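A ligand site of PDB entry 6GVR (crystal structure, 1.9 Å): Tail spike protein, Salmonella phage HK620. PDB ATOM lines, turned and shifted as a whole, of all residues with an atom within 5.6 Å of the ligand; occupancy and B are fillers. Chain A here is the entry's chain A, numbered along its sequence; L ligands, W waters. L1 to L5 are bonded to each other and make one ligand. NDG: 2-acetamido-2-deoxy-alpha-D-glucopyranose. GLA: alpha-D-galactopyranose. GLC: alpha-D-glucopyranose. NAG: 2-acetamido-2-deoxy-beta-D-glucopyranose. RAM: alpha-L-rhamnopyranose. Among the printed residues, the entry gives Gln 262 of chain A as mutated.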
ATOM      1  N   GLY A 101     -27.255   1.217  13.150  1.00  0.00           N
ATOM      2  CA  GLY A 101     -26.673   0.752  11.890  1.00  0.00           C
ATOM      3  C   GLY A 101     -25.587   1.662  11.318  1.00  0.00           C
ATOM      4  O   GLY A 101     -24.877   1.268  10.383  1.00  0.00           O
ATOM      5  N   HIS A 102     -25.453   2.889  11.852  1.00  0.00           N
ATOM      6  CA  HIS A 102     -24.415   3.797  11.493  1.00  0.00           C
ATOM      7  C   HIS A 102     -23.365   3.903  12.582  1.00  0.00           C
ATOM      8  O   HIS A 102     -22.574   4.895  12.586  1.00  0.00           O
ATOM      9  CB  HIS A 102     -25.006   5.196  11.261  1.00  0.00           C
ATOM     10  CG  HIS A 102     -26.116   5.236  10.300  1.00  0.00           C
ATOM     11  ND1 HIS A 102     -25.949   5.507   8.964  1.00  0.00           N
ATOM     12  CD2 HIS A 102     -27.448   5.097  10.481  1.00  0.00           C
ATOM     13  CE1 HIS A 102     -27.105   5.509   8.351  1.00  0.00           C
ATOM     14  NE2 HIS A 102     -28.044   5.258   9.259  1.00  0.00           N
ATOM     15  N   SER A 103     -23.343   2.941  13.520  1.00  0.00           N
ATOM     16  CA  SER A 103     -22.482   2.990  14.742  1.00  0.00           C
ATOM     17  C   SER A 103     -22.651   4.313  15.484  1.00  0.00           C
ATOM     18  O   SER A 103     -21.661   4.826  16.048  1.00  0.00           O
ATOM     19  CB  SER A 103     -20.998   2.806  14.344  1.00  0.00           C
ATOM     20  OG  SER A 103     -20.867   1.551  13.723  1.00  0.00           O
ATOM     21  N   GLN A 132     -19.783   7.028  15.015  1.00  0.00           N
ATOM     22  CA  GLN A 132     -20.206   8.273  14.361  1.00  0.00           C
ATOM     23  C   GLN A 132     -20.896   9.076  15.441  1.00  0.00           C
ATOM     24  O   GLN A 132     -21.895   8.654  15.984  1.00  0.00           O
ATOM     25  CB  GLN A 132     -21.097   7.981  13.149  1.00  0.00           C
ATOM     26  CG  GLN A 132     -20.337   7.313  11.992  1.00  0.00           C
ATOM     27  CD  GLN A 132     -21.136   7.367  10.698  1.00  0.00           C
ATOM     28  OE1 GLN A 132     -21.400   8.455  10.140  1.00  0.00           O
ATOM     29  NE2 GLN A 132     -21.486   6.184  10.154  1.00  0.00           N
ATOM     30  N   PHE A 137     -29.361  10.621  10.498  1.00  0.00           N
ATOM     31  CA  PHE A 137     -30.282   9.621   9.933  1.00  0.00           C
ATOM     32  C   PHE A 137     -31.172   9.133  11.043  1.00  0.00           C
ATOM     33  O   PHE A 137     -30.790   9.159  12.231  1.00  0.00           O
ATOM     34  CB  PHE A 137     -29.584   8.447   9.271  1.00  0.00           C
ATOM     35  CG  PHE A 137     -28.647   8.811   8.109  1.00  0.00           C
ATOM     36  CD1 PHE A 137     -29.127   9.119   6.848  1.00  0.00           C
ATOM     37  CD2 PHE A 137     -27.283   8.807   8.310  1.00  0.00           C
ATOM     38  CE1 PHE A 137     -28.221   9.378   5.809  1.00  0.00           C
ATOM     39  CE2 PHE A 137     -26.381   9.057   7.302  1.00  0.00           C
ATOM     40  CZ  PHE A 137     -26.845   9.307   6.057  1.00  0.00           C
ATOM     41  N   PRO A 142     -30.183   4.442   4.894  1.00  0.00           N
ATOM     42  CA  PRO A 142     -30.400   5.854   4.512  1.00  0.00           C
ATOM     43  C   PRO A 142     -31.484   6.122   3.469  1.00  0.00           C
ATOM     44  O   PRO A 142     -32.194   7.167   3.498  1.00  0.00           O
ATOM     45  CB  PRO A 142     -29.009   6.334   4.060  1.00  0.00           C
ATOM     46  CG  PRO A 142     -28.052   5.208   4.272  1.00  0.00           C
ATOM     47  CD  PRO A 142     -28.768   4.031   4.863  1.00  0.00           C
ATOM     48  N   LEU A 172     -15.401   2.459   9.947  1.00  0.00           N
ATOM     49  CA  LEU A 172     -15.648   3.901   9.688  1.00  0.00           C
ATOM     50  C   LEU A 172     -15.787   4.659  10.994  1.00  0.00           C
ATOM     51  O   LEU A 172     -16.310   4.143  12.004  1.00  0.00           O
ATOM     52  CB  LEU A 172     -16.892   4.112   8.873  1.00  0.00           C
ATOM     53  CG  LEU A 172     -16.913   3.401   7.540  1.00  0.00           C
ATOM     54  CD1 LEU A 172     -18.357   3.426   7.035  1.00  0.00           C
ATOM     55  CD2 LEU A 172     -15.907   3.949   6.532  1.00  0.00           C
ATOM     56  N   ASN A 174     -16.741   8.870  12.201  1.00  0.00           N
ATOM     57  CA  ASN A 174     -17.241  10.232  11.822  1.00  0.00           C
ATOM     58  C   ASN A 174     -17.457  11.054  13.115  1.00  0.00           C
ATOM     59  O   ASN A 174     -17.776  10.534  14.178  1.00  0.00           O
ATOM     60  CB  ASN A 174     -18.551  10.100  10.978  1.00  0.00           C
ATOM     61  CG  ASN A 174     -18.890  11.367  10.166  1.00  0.00           C
ATOM     62  OD1 ASN A 174     -18.162  12.387  10.207  1.00  0.00           O
ATOM     63  ND2 ASN A 174     -19.995  11.312   9.382  1.00  0.00           N
ATOM     64  N   THR A 197     -12.460   8.659   9.701  1.00  0.00           N
ATOM     65  CA  THR A 197     -12.618   8.611   8.268  1.00  0.00           C
ATOM     66  C   THR A 197     -13.000  10.057   7.811  1.00  0.00           C
ATOM     67  O   THR A 197     -12.465  10.576   6.842  1.00  0.00           O
ATOM     68  CB  THR A 197     -13.731   7.689   7.889  1.00  0.00           C
ATOM     69  OG1 THR A 197     -13.504   6.367   8.444  1.00  0.00           O
ATOM     70  CG2 THR A 197     -13.881   7.610   6.412  1.00  0.00           C
ATOM     71  N   TRP A 198     -13.906  10.625   8.539  1.00  0.00           N
ATOM     72  CA  TRP A 198     -14.375  12.022   8.362  1.00  0.00           C
ATOM     73  C   TRP A 198     -14.607  12.699   9.703  1.00  0.00           C
ATOM     74  O   TRP A 198     -14.807  12.019  10.726  1.00  0.00           O
ATOM     75  CB  TRP A 198     -15.694  12.077   7.642  1.00  0.00           C
ATOM     76  CG  TRP A 198     -15.871  11.182   6.416  1.00  0.00           C
ATOM     77  CD1 TRP A 198     -15.361  11.358   5.179  1.00  0.00           C
ATOM     78  CD2 TRP A 198     -16.586   9.930   6.387  1.00  0.00           C
ATOM     79  NE1 TRP A 198     -15.755  10.339   4.350  1.00  0.00           N
ATOM     80  CE2 TRP A 198     -16.524   9.443   5.083  1.00  0.00           C
ATOM     81  CE3 TRP A 198     -17.335   9.220   7.339  1.00  0.00           C
ATOM     82  CZ2 TRP A 198     -17.124   8.264   4.711  1.00  0.00           C
ATOM     83  CZ3 TRP A 198     -17.885   7.981   6.967  1.00  0.00           C
ATOM     84  CH2 TRP A 198     -17.814   7.557   5.661  1.00  0.00           C
ATOM     85  N   THR A 201     -19.879  14.978   7.672  1.00  0.00           N
ATOM     86  CA  THR A 201     -20.423  14.707   6.354  1.00  0.00           C
ATOM     87  C   THR A 201     -21.750  15.397   6.215  1.00  0.00           C
ATOM     88  O   THR A 201     -22.506  15.444   7.189  1.00  0.00           O
ATOM     89  CB  THR A 201     -20.654  13.225   6.123  1.00  0.00           C
ATOM     90  OG1 THR A 201     -21.630  12.699   7.024  1.00  0.00           O
ATOM     91  CG2 THR A 201     -19.373  12.454   6.276  1.00  0.00           C
ATOM     92  N   LEU A 202     -22.040  15.892   5.015  1.00  0.00           N
ATOM     93  CA  LEU A 202     -23.211  16.724   4.766  1.00  0.00           C
ATOM     94  C   LEU A 202     -24.007  16.038   3.678  1.00  0.00           C
ATOM     95  O   LEU A 202     -23.473  15.624   2.670  1.00  0.00           O
ATOM     96  CB  LEU A 202     -22.851  18.105   4.307  1.00  0.00           C
ATOM     97  CG  LEU A 202     -21.859  18.904   5.100  1.00  0.00           C
ATOM     98  CD1 LEU A 202     -21.708  20.282   4.390  1.00  0.00           C
ATOM     99  CD2 LEU A 202     -22.215  19.036   6.559  1.00  0.00           C
ATOM    100  N   GLY A 203     -25.280  15.872   3.889  1.00  0.00           N
ATOM    101  CA  GLY A 203     -26.073  15.229   2.840  1.00  0.00           C
ATOM    102  C   GLY A 203     -25.874  13.703   2.759  1.00  0.00           C
ATOM    103  O   GLY A 203     -25.008  13.100   3.498  1.00  0.00           O
ATOM    104  N   TRP A 204     -26.661  13.109   1.888  1.00  0.00           N
ATOM    105  CA  TRP A 204     -26.544  11.647   1.550  1.00  0.00           C
ATOM    106  C   TRP A 204     -26.937  11.497   0.118  1.00  0.00           C
ATOM    107  O   TRP A 204     -28.127  11.737  -0.221  1.00  0.00           O
ATOM    108  CB  TRP A 204     -27.380  10.753   2.463  1.00  0.00           C
ATOM    109  CG  TRP A 204     -27.316   9.336   2.011  1.00  0.00           C
ATOM    110  CD1 TRP A 204     -26.242   8.518   2.093  1.00  0.00           C
ATOM    111  CD2 TRP A 204     -28.325   8.607   1.259  1.00  0.00           C
ATOM    112  NE1 TRP A 204     -26.518   7.278   1.504  1.00  0.00           N
ATOM    113  CE2 TRP A 204     -27.776   7.322   0.953  1.00  0.00           C
ATOM    114  CE3 TRP A 204     -29.609   8.896   0.839  1.00  0.00           C
ATOM    115  CZ2 TRP A 204     -28.468   6.366   0.253  1.00  0.00           C
ATOM    116  CZ3 TRP A 204     -30.314   7.958   0.133  1.00  0.00           C
ATOM    117  CH2 TRP A 204     -29.738   6.670  -0.136  1.00  0.00           C
ATOM    118  N   ASN A 205     -25.969  11.101  -0.711  1.00  0.00           N
ATOM    119  CA  ASN A 205     -26.178  10.848  -2.132  1.00  0.00           C
ATOM    120  C   ASN A 205     -27.081  11.844  -2.826  1.00  0.00           C
ATOM    121  O   ASN A 205     -28.024  11.519  -3.555  1.00  0.00           O
ATOM    122  CB  ASN A 205     -26.629   9.421  -2.329  1.00  0.00           C
ATOM    123  CG  ASN A 205     -25.564   8.407  -1.959  1.00  0.00           C
ATOM    124  OD1 ASN A 205     -24.436   8.742  -1.482  1.00  0.00           O
ATOM    125  ND2 ASN A 205     -25.977   7.138  -1.997  1.00  0.00           N
ATOM    126  N   ASP A 229      -8.280   5.689   4.981  1.00  0.00           N
ATOM    127  CA  ASP A 229      -8.608   6.845   4.131  1.00  0.00           C
ATOM    128  C   ASP A 229      -9.271   7.901   4.973  1.00  0.00           C
ATOM    129  O   ASP A 229     -10.044   7.574   5.908  1.00  0.00           O
ATOM    130  CB  ASP A 229      -9.568   6.389   3.029  1.00  0.00           C
ATOM    131  CG  ASP A 229      -9.642   7.354   1.892  1.00  0.00           C
ATOM    132  OD1 ASP A 229      -8.960   8.474   1.870  1.00  0.00           O
ATOM    133  OD2 ASP A 229     -10.422   6.957   1.029  1.00  0.00           O
ATOM    134  N   HIS A 230      -9.008   9.155   4.678  1.00  0.00           N
ATOM    135  CA  HIS A 230      -9.611  10.220   5.428  1.00  0.00           C
ATOM    136  C   HIS A 230      -9.949  11.412   4.519  1.00  0.00           C
ATOM    137  O   HIS A 230      -9.157  11.819   3.703  1.00  0.00           O
ATOM    138  CB  HIS A 230      -8.711  10.715   6.557  1.00  0.00           C
ATOM    139  CG  HIS A 230      -9.223  11.941   7.243  1.00  0.00           C
ATOM    140  ND1 HIS A 230      -9.851  11.903   8.485  1.00  0.00           N
ATOM    141  CD2 HIS A 230      -9.147  13.244   6.886  1.00  0.00           C
ATOM    142  CE1 HIS A 230     -10.158  13.150   8.816  1.00  0.00           C
ATOM    143  NE2 HIS A 230      -9.740  13.972   7.865  1.00  0.00           N
ATOM    144  N   SER A 231     -11.163  11.924   4.712  1.00  0.00           N
ATOM    145  CA  SER A 231     -11.589  13.221   4.083  1.00  0.00           C
ATOM    146  C   SER A 231     -12.291  13.991   5.177  1.00  0.00           C
ATOM    147  O   SER A 231     -13.299  13.485   5.709  1.00  0.00           O
ATOM    148  CB  SER A 231     -12.518  12.994   2.891  1.00  0.00           C
ATOM    149  OG  SER A 231     -11.774  12.407   1.811  1.00  0.00           O
ATOM    150  N   TYR A 234     -17.072  15.906   3.952  1.00  0.00           N
ATOM    151  CA  TYR A 234     -17.597  15.304   2.721  1.00  0.00           C
ATOM    152  C   TYR A 234     -18.926  15.987   2.421  1.00  0.00           C
ATOM    153  O   TYR A 234     -19.901  15.897   3.197  1.00  0.00           O
ATOM    154  CB  TYR A 234     -17.844  13.803   2.902  1.00  0.00           C
ATOM    155  CG  TYR A 234     -17.913  12.922   1.667  1.00  0.00           C
ATOM    156  CD1 TYR A 234     -18.999  12.980   0.800  1.00  0.00           C
ATOM    157  CD2 TYR A 234     -16.914  11.980   1.369  1.00  0.00           C
ATOM    158  CE1 TYR A 234     -19.065  12.145  -0.316  1.00  0.00           C
ATOM    159  CE2 TYR A 234     -16.989  11.143   0.271  1.00  0.00           C
ATOM    160  CZ  TYR A 234     -18.108  11.176  -0.547  1.00  0.00           C
ATOM    161  OH  TYR A 234     -18.196  10.307  -1.609  1.00  0.00           O
ATOM    162  N   ASN A 236     -22.042  16.121   0.338  1.00  0.00           N
ATOM    163  CA  ASN A 236     -22.835  15.199  -0.529  1.00  0.00           C
ATOM    164  C   ASN A 236     -24.294  15.634  -0.679  1.00  0.00           C
ATOM    165  O   ASN A 236     -25.219  14.868  -1.000  1.00  0.00           O
ATOM    166  CB  ASN A 236     -22.733  13.787  -0.004  1.00  0.00           C
ATOM    167  CG  ASN A 236     -22.883  12.720  -1.081  1.00  0.00           C
ATOM    168  OD1 ASN A 236     -22.953  13.007  -2.270  1.00  0.00           O
ATOM    169  ND2 ASN A 236     -22.987  11.404  -0.626  1.00  0.00           N
ATOM    170  N   GLN A 262     -14.335  16.995   0.310  1.00  0.00           N
ATOM    171  CA  GLN A 262     -14.922  16.331  -0.868  1.00  0.00           C
ATOM    172  C   GLN A 262     -16.090  17.206  -1.351  1.00  0.00           C
ATOM    173  O   GLN A 262     -17.020  17.351  -0.566  1.00  0.00           O
ATOM    174  CB  GLN A 262     -15.468  14.895  -0.513  1.00  0.00           C
ATOM    175  CG  GLN A 262     -14.365  13.935  -0.004  1.00  0.00           C
ATOM    176  CD  GLN A 262     -13.403  13.355  -1.080  1.00  0.00           C
ATOM    177  OE1 GLN A 262     -12.219  13.062  -0.748  1.00  0.00           O
ATOM    178  NE2 GLN A 262     -13.876  13.123  -2.311  1.00  0.00           N
ATOM    179  N   HIS A 264     -19.059  16.905  -3.845  1.00  0.00           N
ATOM    180  CA  HIS A 264     -19.591  15.807  -4.641  1.00  0.00           C
ATOM    181  C   HIS A 264     -20.963  16.051  -5.181  1.00  0.00           C
ATOM    182  O   HIS A 264     -21.557  15.083  -5.715  1.00  0.00           O
ATOM    183  CB  HIS A 264     -19.609  14.522  -3.852  1.00  0.00           C
ATOM    184  CG  HIS A 264     -18.307  13.835  -3.795  1.00  0.00           C
ATOM    185  ND1 HIS A 264     -18.192  12.464  -3.876  1.00  0.00           N
ATOM    186  CD2 HIS A 264     -17.043  14.307  -3.724  1.00  0.00           C
ATOM    187  CE1 HIS A 264     -16.914  12.119  -3.816  1.00  0.00           C
ATOM    188  NE2 HIS A 264     -16.199  13.202  -3.652  1.00  0.00           N
ATOM    189  N   TYR A 283     -11.206  16.904  -3.487  1.00  0.00           N
ATOM    190  CA  TYR A 283     -11.722  16.205  -4.652  1.00  0.00           C
ATOM    191  C   TYR A 283     -13.003  16.922  -5.117  1.00  0.00           C
ATOM    192  O   TYR A 283     -13.818  17.310  -4.285  1.00  0.00           O
ATOM    193  CB  TYR A 283     -12.085  14.776  -4.335  1.00  0.00           C
ATOM    194  CG  TYR A 283     -10.920  13.817  -4.168  1.00  0.00           C
ATOM    195  CD1 TYR A 283     -10.247  13.723  -2.946  1.00  0.00           C
ATOM    196  CD2 TYR A 283     -10.532  12.949  -5.223  1.00  0.00           C
ATOM    197  CE1 TYR A 283      -9.225  12.745  -2.744  1.00  0.00           C
ATOM    198  CE2 TYR A 283      -9.450  12.034  -5.030  1.00  0.00           C
ATOM    199  CZ  TYR A 283      -8.808  11.955  -3.800  1.00  0.00           C
ATOM    200  OH  TYR A 283      -7.782  11.027  -3.627  1.00  0.00           O
ATOM    201  N   VAL A 285     -15.828  15.926  -7.634  1.00  0.00           N
ATOM    202  CA  VAL A 285     -16.104  14.612  -8.275  1.00  0.00           C
ATOM    203  C   VAL A 285     -17.601  14.416  -8.381  1.00  0.00           C
ATOM    204  O   VAL A 285     -18.279  14.625  -7.364  1.00  0.00           O
ATOM    205  CB  VAL A 285     -15.525  13.418  -7.440  1.00  0.00           C
ATOM    206  CG1 VAL A 285     -16.042  12.057  -7.964  1.00  0.00           C
ATOM    207  CG2 VAL A 285     -14.018  13.385  -7.483  1.00  0.00           C
ATOM    208  N   HIS A 287     -19.799  11.218  -8.569  1.00  0.00           N
ATOM    209  CA  HIS A 287     -19.870   9.738  -8.564  1.00  0.00           C
ATOM    210  C   HIS A 287     -21.302   9.348  -9.038  1.00  0.00           C
ATOM    211  O   HIS A 287     -22.283   9.662  -8.382  1.00  0.00           O
ATOM    212  CB  HIS A 287     -19.678   9.157  -7.173  1.00  0.00           C
ATOM    213  CG  HIS A 287     -18.266   9.085  -6.655  1.00  0.00           C
ATOM    214  ND1 HIS A 287     -17.222   8.577  -7.384  1.00  0.00           N
ATOM    215  CD2 HIS A 287     -17.794   9.236  -5.385  1.00  0.00           C
ATOM    216  CE1 HIS A 287     -16.126   8.557  -6.634  1.00  0.00           C
ATOM    217  NE2 HIS A 287     -16.438   8.986  -5.424  1.00  0.00           N
ATOM    218  N   ALA A 289     -22.747   6.710  -8.489  1.00  0.00           N
ATOM    219  CA  ALA A 289     -23.351   6.080  -7.350  1.00  0.00           C
ATOM    220  C   ALA A 289     -23.985   6.986  -6.311  1.00  0.00           C
ATOM    221  O   ALA A 289     -24.751   6.514  -5.452  1.00  0.00           O
ATOM    222  CB  ALA A 289     -22.355   5.123  -6.693  1.00  0.00           C
ATOM    223  N   GLU A 290     -23.735   8.287  -6.370  1.00  0.00           N
ATOM    224  CA  GLU A 290     -24.232   9.209  -5.414  1.00  0.00           C
ATOM    225  C   GLU A 290     -25.210  10.160  -6.039  1.00  0.00           C
ATOM    226  O   GLU A 290     -25.463  11.272  -5.518  1.00  0.00           O
ATOM    227  CB  GLU A 290     -23.010  10.039  -4.836  1.00  0.00           C
ATOM    228  CG  GLU A 290     -22.027   9.166  -4.066  1.00  0.00           C
ATOM    229  CD  GLU A 290     -20.898   9.957  -3.451  1.00  0.00           C
ATOM    230  OE1 GLU A 290     -20.496  10.972  -4.099  1.00  0.00           O
ATOM    231  OE2 GLU A 290     -20.414   9.519  -2.392  1.00  0.00           O
ATOM    232  N   PRO A 359     -10.589  10.266 -10.776  1.00  0.00           N
ATOM    233  CA  PRO A 359      -9.912   9.889  -9.483  1.00  0.00           C
ATOM    234  C   PRO A 359      -9.432   8.364  -9.503  1.00  0.00           C
ATOM    235  O   PRO A 359      -8.222   8.036  -9.433  1.00  0.00           O
ATOM    236  CB  PRO A 359     -11.052  10.112  -8.440  1.00  0.00           C
ATOM    237  CG  PRO A 359     -12.386   9.955  -9.231  1.00  0.00           C
ATOM    238  CD  PRO A 359     -12.035   9.872 -10.723  1.00  0.00           C
HETATM  239  C1  NDG L   1     -11.798   9.976  -1.357  1.00  0.00           C
HETATM  240  C2  NDG L   1     -13.049   9.424  -0.641  1.00  0.00           C
HETATM  241  C3  NDG L   1     -13.719   8.334  -1.511  1.00  0.00           C
HETATM  242  C4  NDG L   1     -14.009   8.925  -2.897  1.00  0.00           C
HETATM  243  C5  NDG L   1     -12.721   9.487  -3.535  1.00  0.00           C
HETATM  244  C6  NDG L   1     -12.906  10.227  -4.818  1.00  0.00           C
HETATM  245  C7  NDG L   1     -13.242   9.375   1.838  1.00  0.00           C
HETATM  246  C8  NDG L   1     -12.634   8.880   3.096  1.00  0.00           C
HETATM  247  O5  NDG L   1     -12.115  10.430  -2.677  1.00  0.00           O
HETATM  248  O3  NDG L   1     -14.986   7.950  -0.881  1.00  0.00           O
HETATM  249  O4  NDG L   1     -14.683   8.027  -3.799  1.00  0.00           O
HETATM  250  O6  NDG L   1     -13.690  11.382  -4.433  1.00  0.00           O
HETATM  251  O7  NDG L   1     -14.255  10.088   1.859  1.00  0.00           O
HETATM  252  N2  NDG L   1     -12.662   8.966   0.683  1.00  0.00           N
HETATM  253  O1  NDG L   1     -10.863   8.954  -1.525  1.00  0.00           O
HETATM  254  C1  GLA L   2     -15.353   6.583  -1.085  1.00  0.00           C
HETATM  255  C2  GLA L   2     -16.851   6.531  -0.896  1.00  0.00           C
HETATM  256  C3  GLA L   2     -17.284   6.871   0.549  1.00  0.00           C
HETATM  257  C4  GLA L   2     -16.455   6.076   1.561  1.00  0.00           C
HETATM  258  C5  GLA L   2     -14.954   6.237   1.257  1.00  0.00           C
HETATM  259  C6  GLA L   2     -14.006   5.443   2.140  1.00  0.00           C
HETATM  260  O2  GLA L   2     -17.483   7.454  -1.814  1.00  0.00           O
HETATM  261  O3  GLA L   2     -18.687   6.570   0.633  1.00  0.00           O
HETATM  262  O4  GLA L   2     -16.793   4.667   1.449  1.00  0.00           O
HETATM  263  O5  GLA L   2     -14.697   5.872  -0.114  1.00  0.00           O
HETATM  264  O6  GLA L   2     -14.299   5.769   3.488  1.00  0.00           O
HETATM  265  C1  GLC L   3     -17.046   4.079   2.759  1.00  0.00           C
HETATM  266  C2  GLC L   3     -17.140   2.538   2.621  1.00  0.00           C
HETATM  267  C3  GLC L   3     -18.306   2.087   1.739  1.00  0.00           C
HETATM  268  C4  GLC L   3     -19.520   2.656   2.369  1.00  0.00           C
HETATM  269  C5  GLC L   3     -19.412   4.179   2.468  1.00  0.00           C
HETATM  270  C6  GLC L   3     -20.654   4.834   3.091  1.00  0.00           C
HETATM  271  O2  GLC L   3     -15.971   2.055   2.098  1.00  0.00           O
HETATM  272  O3  GLC L   3     -18.395   0.678   1.830  1.00  0.00           O
HETATM  273  O4  GLC L   3     -20.640   2.222   1.650  1.00  0.00           O
HETATM  274  O5  GLC L   3     -18.264   4.532   3.299  1.00  0.00           O
HETATM  275  O6  GLC L   3     -20.908   4.370   4.455  1.00  0.00           O
HETATM  276  C1  NAG L   4     -19.485   7.744   0.785  1.00  0.00           C
HETATM  277  C2  NAG L   4     -20.911   7.398   0.385  1.00  0.00           C
HETATM  278  C3  NAG L   4     -21.873   8.550   0.629  1.00  0.00           C
HETATM  279  C4  NAG L   4     -21.686   9.195   1.966  1.00  0.00           C
HETATM  280  C5  NAG L   4     -20.233   9.506   2.103  1.00  0.00           C
HETATM  281  C6  NAG L   4     -19.970  10.277   3.354  1.00  0.00           C
HETATM  282  C7  NAG L   4     -21.250   5.831  -1.437  1.00  0.00           C
HETATM  283  C8  NAG L   4     -21.145   5.531  -2.920  1.00  0.00           C
HETATM  284  N2  NAG L   4     -20.880   7.044  -1.005  1.00  0.00           N
HETATM  285  O3  NAG L   4     -23.144   7.985   0.569  1.00  0.00           O
HETATM  286  O4  NAG L   4     -22.413  10.429   1.944  1.00  0.00           O
HETATM  287  O5  NAG L   4     -19.453   8.283   2.109  1.00  0.00           O
HETATM  288  O6  NAG L   4     -20.233   9.421   4.421  1.00  0.00           O
HETATM  289  O7  NAG L   4     -21.734   5.008  -0.681  1.00  0.00           O
HETATM  290  C1  RAM L   5     -22.194   3.705   4.527  1.00  0.00           C
HETATM  291  C2  RAM L   5     -22.257   2.975   5.872  1.00  0.00           C
HETATM  292  C3  RAM L   5     -22.340   3.934   7.054  1.00  0.00           C
HETATM  293  C4  RAM L   5     -23.441   4.975   6.780  1.00  0.00           C
HETATM  294  C5  RAM L   5     -23.322   5.581   5.365  1.00  0.00           C
HETATM  295  C6  RAM L   5     -24.469   6.536   4.980  1.00  0.00           C
HETATM  296  O2  RAM L   5     -23.414   2.166   5.752  1.00  0.00           O
HETATM  297  O3  RAM L   5     -22.538   3.191   8.290  1.00  0.00           O
HETATM  298  O4  RAM L   5     -23.438   5.938   7.849  1.00  0.00           O
HETATM  299  O5  RAM L   5     -23.307   4.572   4.348  1.00  0.00           O
HETATM  300  O   HOH W   1     -14.862   0.785   4.089  1.00  0.00           O
HETATM  301  O   HOH W   2     -22.410  10.200   6.075  1.00  0.00           O
HETATM  302  O   HOH W   3     -17.620   5.833  -4.056  1.00  0.00           O
HETATM  303  O   HOH W   4     -26.116   2.248   7.432  1.00  0.00           O
HETATM  304  O   HOH W   5     -20.545   2.857  10.457  1.00  0.00           O
HETATM  305  O   HOH W   6     -22.499   0.517   8.566  1.00  0.00           O
HETATM  306  O   HOH W   7     -24.144   5.486   1.666  1.00  0.00           O
HETATM  307  O   HOH W   8     -22.924   8.541   8.184  1.00  0.00           O
HETATM  308  O   HOH W   9     -24.155  10.469   4.036  1.00  0.00           O
HETATM  309  O   HOH W  10      -8.261   9.268  -1.393  1.00  0.00           O
HETATM  310  O   HOH W  11     -22.834   0.474   3.744  1.00  0.00           O
HETATM  311  O   HOH W  12     -20.054  -0.720   0.139  1.00  0.00           O
HETATM  312  O   HOH W  13     -24.477   4.870  -1.012  1.00  0.00           O
HETATM  313  O   HOH W  14     -13.600   5.911  -4.748  1.00  0.00           O
HETATM  314  O   HOH W  15     -15.449   2.944  -0.638  1.00  0.00           O
HETATM  315  O   HOH W  16     -12.399   4.338   4.824  1.00  0.00           O
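OD2 of Asp 229 is in hydrogen-bond range of N2 of NDG L1. An oxygen (O6) of NDG L1 sits at hydrogen-bond distance from the side-chain amide nitrogen (NE2) of Gln 262, at 2.8 Å. An oxygen (O4) of RAM L5 sits at hydrogen-bond distance from the side-chain amide nitrogen (NE2) of Gln 132 (3.0 Å). An oxygen (O4) of NAG L4 lies within hydrogen-bond range of the side-chain amide nitrogen of Asn 236. A ring nitrogen (NE2) of His 264 sits at hydrogen-bond distance from an oxygen (O6) of NDG L1. OD1 of Asn 205 sits at hydrogen-bond distance from O3 of NAG L4 (2.5 Å). The side-chain carboxylate (OE2) of Glu 290 is in hydrogen-bond range of a nitrogen (N2) of NAG L4, 2.9 Å away. O7 of NDG L1 sits close to OG of Ser 231. A ring nitrogen (ND1) of His 102 sits at hydrogen-bond distance from an oxygen (O4) of RAM L5 (2.8 Å). OH of Tyr 234 sits at hydrogen-bond distance from O2 of GLA L2 (2.9 Å). NE2 of His 287 sits at hydrogen-bond distance from O4 of NDG L1 (2.6 Å). NE1 of Trp 198 lies within hydrogen-bond range of O7 of NDG L1, 2.9 Å away.
O of Gly 101 touches O3 of RAM L5, 3.7 Å away. Phe 137 touches the ligand. Pro 142 touches the ligand. CD1 of Leu 172 touches O6 of GLC L3, at 3.7 Å. CG2 of Thr 197 touches O6 of GLA L2, at 3.5 Å. CG2 of Thr 201 touches O6 of NAG L4, at 3.7 Å. Trp 204 touches the ligand. His 230 touches the ligand. CD2 of Tyr 283 touches O6 of NDG L1 (3.6 Å). CG2 of Val 285 touches O6 of NDG L1, 3.7 Å away. Ala 289 touches the ligand. Hydrophobic or aromatic side chains within 4 Å of the ligand: His 102, Phe 137, Pro 142, Leu 172, Trp 198, Trp 204, Tyr 234, His 264, Tyr 283, Val 285, His 287 and Ala 289. The nearest printed residue that does not touch the ligand is Gly 203 (4.04 Å).
Water W8 bridges OE1 of Gln 132 (2.5 Å) and O4 of RAM L5 (2.7 Å). Water W6 lies within hydrogen-bond range of O3 of RAM L5 and O of Gly 101. Water W13 bridges an oxygen (O7) of NAG L4 and the side-chain amide nitrogen (ND2) of Asn 205. Water W2 bridges OG1 of Thr 201 (2.8 Å) and O6 of NAG L4 (2.8 Å). Water W5 bridges O3 of RAM L5 (3.0 Å) and NE2 of Gln 132 (3.5 Å). Water W4 bridges O2 of RAM L5 (3.2 Å) and O of Gly 101 (3.3 Å).
N of Gln 132 is in hydrogen-bond range of O of Ser 103, at 3.1 Å. OH of Tyr 234 lies within hydrogen-bond range of OE2 of Glu 290, 2.5 Å away. O of Tyr 234 is in hydrogen-bond range of N of Leu 202 (2.8 Å). O of Thr 197 sits at hydrogen-bond distance from N of Ser 231 (2.8 Å). The side-chain amide nitrogen (NE2) of Gln 132 is in hydrogen-bond range of the backbone carbonyl oxygen (O) of His 102 (3.0 Å). NE2 of Gln 262 sits at hydrogen-bond distance from NE2 of His 264 (2.7 Å). OE1 of Gln 132 lies within hydrogen-bond range of ND2 of Asn 174 (3.3 Å). ND1 of His 264 sits at hydrogen-bond distance from OE1 of Glu 290.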
